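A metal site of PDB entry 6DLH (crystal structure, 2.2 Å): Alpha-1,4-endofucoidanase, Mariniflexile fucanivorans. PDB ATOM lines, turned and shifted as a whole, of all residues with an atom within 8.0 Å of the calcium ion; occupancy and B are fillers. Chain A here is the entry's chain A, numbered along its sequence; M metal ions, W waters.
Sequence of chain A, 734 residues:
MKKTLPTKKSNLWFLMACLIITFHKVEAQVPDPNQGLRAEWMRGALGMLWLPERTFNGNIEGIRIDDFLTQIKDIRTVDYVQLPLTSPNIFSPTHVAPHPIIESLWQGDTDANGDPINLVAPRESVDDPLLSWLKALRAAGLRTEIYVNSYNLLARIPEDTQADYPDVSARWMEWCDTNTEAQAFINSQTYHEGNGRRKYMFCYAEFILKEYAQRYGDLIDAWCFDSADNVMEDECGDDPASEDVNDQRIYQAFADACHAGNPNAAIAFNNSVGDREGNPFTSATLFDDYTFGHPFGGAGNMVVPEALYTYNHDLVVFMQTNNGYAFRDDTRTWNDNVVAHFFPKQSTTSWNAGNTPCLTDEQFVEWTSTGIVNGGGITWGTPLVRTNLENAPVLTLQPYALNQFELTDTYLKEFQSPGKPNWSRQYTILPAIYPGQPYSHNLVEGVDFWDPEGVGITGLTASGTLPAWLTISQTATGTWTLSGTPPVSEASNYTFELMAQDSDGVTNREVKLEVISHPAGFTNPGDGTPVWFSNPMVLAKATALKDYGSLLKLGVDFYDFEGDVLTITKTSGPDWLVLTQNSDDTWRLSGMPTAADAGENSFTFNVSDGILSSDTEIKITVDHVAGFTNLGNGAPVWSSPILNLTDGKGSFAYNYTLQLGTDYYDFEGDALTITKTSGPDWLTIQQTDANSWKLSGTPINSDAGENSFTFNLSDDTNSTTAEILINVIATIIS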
ATOM      1  N   SER A 417     -29.359 -20.372   1.470  1.00  0.00           N
ATOM      2  CA  SER A 417     -28.650 -20.548   0.211  1.00  0.00           C
ATOM      3  C   SER A 417     -27.773 -19.332  -0.052  1.00  0.00           C
ATOM      4  O   SER A 417     -28.181 -18.428  -0.779  1.00  0.00           O
ATOM      5  CB  SER A 417     -29.582 -20.760  -0.949  1.00  0.00           C
ATOM      6  OG  SER A 417     -30.642 -21.611  -0.585  1.00  0.00           O
ATOM      7  N   PRO A 418     -26.564 -19.268   0.543  1.00  0.00           N
ATOM      8  CA  PRO A 418     -25.699 -18.088   0.396  1.00  0.00           C
ATOM      9  C   PRO A 418     -25.186 -17.884  -1.033  1.00  0.00           C
ATOM     10  O   PRO A 418     -25.341 -18.772  -1.877  1.00  0.00           O
ATOM     11  CB  PRO A 418     -24.543 -18.389   1.382  1.00  0.00           C
ATOM     12  CG  PRO A 418     -25.117 -19.445   2.325  1.00  0.00           C
ATOM     13  CD  PRO A 418     -25.993 -20.291   1.422  1.00  0.00           C
ATOM     14  N   GLY A 419     -24.622 -16.702  -1.297  1.00  0.00           N
ATOM     15  CA  GLY A 419     -23.930 -16.433  -2.558  1.00  0.00           C
ATOM     16  C   GLY A 419     -24.803 -15.722  -3.588  1.00  0.00           C
ATOM     17  O   GLY A 419     -24.948 -14.511  -3.562  1.00  0.00           O
ATOM     18  N   LYS A 420     -25.346 -16.515  -4.525  1.00  0.00           N
ATOM     19  CA  LYS A 420     -26.177 -16.005  -5.600  1.00  0.00           C
ATOM     20  C   LYS A 420     -27.522 -15.546  -5.028  1.00  0.00           C
ATOM     21  O   LYS A 420     -27.883 -15.910  -3.916  1.00  0.00           O
ATOM     22  CB  LYS A 420     -26.380 -17.085  -6.667  1.00  0.00           C
ATOM     23  CG  LYS A 420     -25.156 -17.346  -7.544  1.00  0.00           C
ATOM     24  CD  LYS A 420     -25.305 -18.546  -8.460  1.00  0.00           C
ATOM     25  CE  LYS A 420     -24.083 -18.819  -9.320  1.00  0.00           C
ATOM     26  NZ  LYS A 420     -22.824 -18.705  -8.552  1.00  0.00           N
ATOM     27  N   PRO A 421     -28.288 -14.703  -5.762  1.00  0.00           N
ATOM     28  CA  PRO A 421     -29.588 -14.214  -5.291  1.00  0.00           C
ATOM     29  C   PRO A 421     -30.595 -15.308  -4.944  1.00  0.00           C
ATOM     30  O   PRO A 421     -30.627 -16.359  -5.578  1.00  0.00           O
ATOM     31  CB  PRO A 421     -30.125 -13.402  -6.469  1.00  0.00           C
ATOM     32  CG  PRO A 421     -28.880 -12.950  -7.211  1.00  0.00           C
ATOM     33  CD  PRO A 421     -27.915 -14.103  -7.059  1.00  0.00           C
ATOM     34  N   ASN A 422     -31.436 -15.025  -3.941  1.00  0.00           N
ATOM     35  CA  ASN A 422     -32.574 -15.875  -3.622  1.00  0.00           C
ATOM     36  C   ASN A 422     -33.864 -15.181  -4.070  1.00  0.00           C
ATOM     37  O   ASN A 422     -34.031 -13.985  -3.853  1.00  0.00           O
ATOM     38  CB  ASN A 422     -32.653 -16.208  -2.130  1.00  0.00           C
ATOM     39  CG  ASN A 422     -31.425 -16.898  -1.582  1.00  0.00           C
ATOM     40  OD1 ASN A 422     -31.227 -16.926  -0.368  1.00  0.00           O
ATOM     41  ND2 ASN A 422     -30.583 -17.450  -2.440  1.00  0.00           N
ATOM     42  N   TRP A 450     -33.212 -11.085  -3.282  1.00  0.00           N
ATOM     43  CA  TRP A 450     -32.225 -10.420  -2.435  1.00  0.00           C
ATOM     44  C   TRP A 450     -30.881 -11.115  -2.586  1.00  0.00           C
ATOM     45  O   TRP A 450     -30.796 -12.265  -3.019  1.00  0.00           O
ATOM     46  CB  TRP A 450     -32.692 -10.366  -0.978  1.00  0.00           C
ATOM     47  CG  TRP A 450     -32.896 -11.711  -0.382  1.00  0.00           C
ATOM     48  CD1 TRP A 450     -31.967 -12.499   0.233  1.00  0.00           C
ATOM     49  CD2 TRP A 450     -34.127 -12.463  -0.365  1.00  0.00           C
ATOM     50  NE1 TRP A 450     -32.525 -13.675   0.632  1.00  0.00           N
ATOM     51  CE2 TRP A 450     -33.848 -13.694   0.278  1.00  0.00           C
ATOM     52  CE3 TRP A 450     -35.421 -12.223  -0.837  1.00  0.00           C
ATOM     53  CZ2 TRP A 450     -34.826 -14.671   0.457  1.00  0.00           C
ATOM     54  CZ3 TRP A 450     -36.392 -13.188  -0.659  1.00  0.00           C
ATOM     55  CH2 TRP A 450     -36.091 -14.397  -0.010  1.00  0.00           C
ATOM     56  N   ASP A 451     -29.820 -10.365  -2.247  1.00  0.00           N
ATOM     57  CA  ASP A 451     -28.476 -10.900  -2.115  1.00  0.00           C
ATOM     58  C   ASP A 451     -28.284 -11.366  -0.679  1.00  0.00           C
ATOM     59  O   ASP A 451     -28.326 -10.547   0.240  1.00  0.00           O
ATOM     60  CB  ASP A 451     -27.451  -9.851  -2.575  1.00  0.00           C
ATOM     61  CG  ASP A 451     -26.059  -9.988  -1.960  1.00  0.00           C
ATOM     62  OD1 ASP A 451     -25.751 -11.064  -1.424  1.00  0.00           O
ATOM     63  OD2 ASP A 451     -25.312  -8.992  -2.012  1.00  0.00           O
ATOM     64  N   PRO A 452     -28.099 -12.685  -0.437  1.00  0.00           N
ATOM     65  CA  PRO A 452     -27.969 -13.202   0.925  1.00  0.00           C
ATOM     66  C   PRO A 452     -26.962 -12.443   1.780  1.00  0.00           C
ATOM     67  O   PRO A 452     -27.199 -12.240   2.975  1.00  0.00           O
ATOM     68  CB  PRO A 452     -27.511 -14.642   0.681  1.00  0.00           C
ATOM     69  CG  PRO A 452     -28.194 -15.011  -0.619  1.00  0.00           C
ATOM     70  CD  PRO A 452     -28.077 -13.753  -1.450  1.00  0.00           C
ATOM     71  N   GLU A 453     -25.867 -11.988   1.168  1.00  0.00           N
ATOM     72  CA  GLU A 453     -24.763 -11.364   1.894  1.00  0.00           C
ATOM     73  C   GLU A 453     -25.013  -9.863   2.048  1.00  0.00           C
ATOM     74  O   GLU A 453     -24.271  -9.186   2.775  1.00  0.00           O
ATOM     75  CB  GLU A 453     -23.425 -11.649   1.219  1.00  0.00           C
ATOM     76  CG  GLU A 453     -22.924 -13.063   1.448  1.00  0.00           C
ATOM     77  CD  GLU A 453     -23.670 -14.114   0.633  1.00  0.00           C
ATOM     78  OE1 GLU A 453     -24.149 -13.772  -0.448  1.00  0.00           O
ATOM     79  OE2 GLU A 453     -23.773 -15.255   1.097  1.00  0.00           O
ATOM     80  N   GLY A 454     -26.029  -9.351   1.356  1.00  0.00           N
ATOM     81  CA  GLY A 454     -26.534  -8.004   1.623  1.00  0.00           C
ATOM     82  C   GLY A 454     -25.713  -6.902   0.962  1.00  0.00           C
ATOM     83  O   GLY A 454     -25.812  -5.748   1.369  1.00  0.00           O
ATOM     84  N   VAL A 455     -24.910  -7.255  -0.063  1.00  0.00           N
ATOM     85  CA  VAL A 455     -24.209  -6.258  -0.843  1.00  0.00           C
ATOM     86  C   VAL A 455     -25.231  -5.570  -1.745  1.00  0.00           C
ATOM     87  O   VAL A 455     -25.402  -4.349  -1.676  1.00  0.00           O
ATOM     88  CB  VAL A 455     -23.013  -6.837  -1.640  1.00  0.00           C
ATOM     89  CG1 VAL A 455     -22.250  -5.756  -2.389  1.00  0.00           C
ATOM     90  CG2 VAL A 455     -22.062  -7.635  -0.751  1.00  0.00           C
ATOM     91  N   GLY A 456     -25.931  -6.365  -2.557  1.00  0.00           N
ATOM     92  CA  GLY A 456     -27.075  -5.890  -3.298  1.00  0.00           C
ATOM     93  C   GLY A 456     -27.278  -6.642  -4.605  1.00  0.00           C
ATOM     94  O   GLY A 456     -26.367  -7.311  -5.089  1.00  0.00           O
ATOM     95  N   GLN A 501     -29.248 -10.807 -10.338  1.00  0.00           N
ATOM     96  CA  GLN A 501     -27.805 -10.831 -10.314  1.00  0.00           C
ATOM     97  C   GLN A 501     -27.298 -10.118  -9.058  1.00  0.00           C
ATOM     98  O   GLN A 501     -27.879  -9.105  -8.645  1.00  0.00           O
ATOM     99  CB  GLN A 501     -27.241 -10.147 -11.565  1.00  0.00           C
ATOM    100  CG  GLN A 501     -25.727 -10.255 -11.675  1.00  0.00           C
ATOM    101  CD  GLN A 501     -25.117  -9.477 -12.817  1.00  0.00           C
ATOM    102  OE1 GLN A 501     -25.471  -8.322 -13.065  1.00  0.00           O
ATOM    103  NE2 GLN A 501     -24.168 -10.086 -13.501  1.00  0.00           N
ATOM    104  N   ASP A 502     -26.231 -10.669  -8.483  1.00  0.00           N
ATOM    105  CA  ASP A 502     -25.398  -9.962  -7.517  1.00  0.00           C
ATOM    106  C   ASP A 502     -23.927 -10.204  -7.874  1.00  0.00           C
ATOM    107  O   ASP A 502     -23.624 -10.817  -8.901  1.00  0.00           O
ATOM    108  CB  ASP A 502     -25.765 -10.316  -6.069  1.00  0.00           C
ATOM    109  CG  ASP A 502     -25.598 -11.782  -5.674  1.00  0.00           C
ATOM    110  OD1 ASP A 502     -25.019 -12.569  -6.466  1.00  0.00           O
ATOM    111  OD2 ASP A 502     -26.050 -12.131  -4.544  1.00  0.00           O
ATOM    112  N   SER A 503     -23.023  -9.736  -7.020  1.00  0.00           N
ATOM    113  CA  SER A 503     -21.600  -9.795  -7.302  1.00  0.00           C
ATOM    114  C   SER A 503     -21.130 -11.231  -7.526  1.00  0.00           C
ATOM    115  O   SER A 503     -20.054 -11.441  -8.070  1.00  0.00           O
ATOM    116  CB  SER A 503     -20.806  -9.125  -6.213  1.00  0.00           C
ATOM    117  OG  SER A 503     -20.936  -9.854  -4.994  1.00  0.00           O
ATOM    118  N   ASP A 504     -21.967 -12.212  -7.121  1.00  0.00           N
ATOM    119  CA  ASP A 504     -21.591 -13.611  -7.031  1.00  0.00           C
ATOM    120  C   ASP A 504     -22.146 -14.419  -8.210  1.00  0.00           C
ATOM    121  O   ASP A 504     -21.703 -15.541  -8.446  1.00  0.00           O
ATOM    122  CB  ASP A 504     -22.048 -14.228  -5.695  1.00  0.00           C
ATOM    123  CG  ASP A 504     -21.381 -15.552  -5.347  1.00  0.00           C
ATOM    124  OD1 ASP A 504     -20.182 -15.535  -4.990  1.00  0.00           O
ATOM    125  OD2 ASP A 504     -22.058 -16.602  -5.458  1.00  0.00           O
ATOM    126  N   GLY A 505     -23.140 -13.881  -8.925  1.00  0.00           N
ATOM    127  CA  GLY A 505     -23.715 -14.601 -10.055  1.00  0.00           C
ATOM    128  C   GLY A 505     -25.222 -14.376 -10.196  1.00  0.00           C
ATOM    129  O   GLY A 505     -25.751 -13.413  -9.653  1.00  0.00           O
HETATM  130 CA    CA M   1     -24.098 -12.793  -2.580  1.00  0.00          CA
HETATM  131  O   HOH W   1     -23.227 -10.623  -3.538  1.00  0.00           O
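Water W1 bridges the side-chain hydroxyl of Ser 503 (2.8 Å) and the side-chain carboxylate of Asp 451 (3.1 Å).
O of Gly 419 is bound to the calcium ion (2.2 Å).
The calcium ion is bound by OE1 of Glu 453 (2.3 Å).
Water W1 is bound to the calcium ion, 2.5 Å away.
The side-chain carboxylate (OD1) of Asp 451 is bound to the calcium ion (2.7 Å).
The side-chain carboxylate (OD2) of Asp 502 is bound to the calcium ion (2.8 Å).
OD2 of Asp 451 sits close to N of Gly 454, at 3.5 Å.
The side-chain carboxylate (OD2) of Asp 451 sits at hydrogen-bond distance from the backbone NH (N) of Val 455 (2.6 Å).
The backbone NH of Gly 456 sits at hydrogen-bond distance from the side-chain carboxylate of Asp 451 (2.8 Å).
The side-chain carboxylate (OD1) of Asp 502 lies close to the backbone NH (N) of Asp 504 (3.1 Å).
OD1 of Asp 502 sits at hydrogen-bond distance from N of Gly 505, at 3.4 Å.
The side-chain amino group (NZ) of Lys 420 is in salt-bridge range of the side-chain carboxylate (OD2) of Asp 504.
Asp 504 touches the calcium ion (CB to CA, 3.996 Å).
Within 4 Å of the calcium ion: Gly 419, Asp 451, Glu 453, Asp 502 and Asp 504.
The nearest printed residue that does not touch the calcium ion is Pro 452 (4.2 Å).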
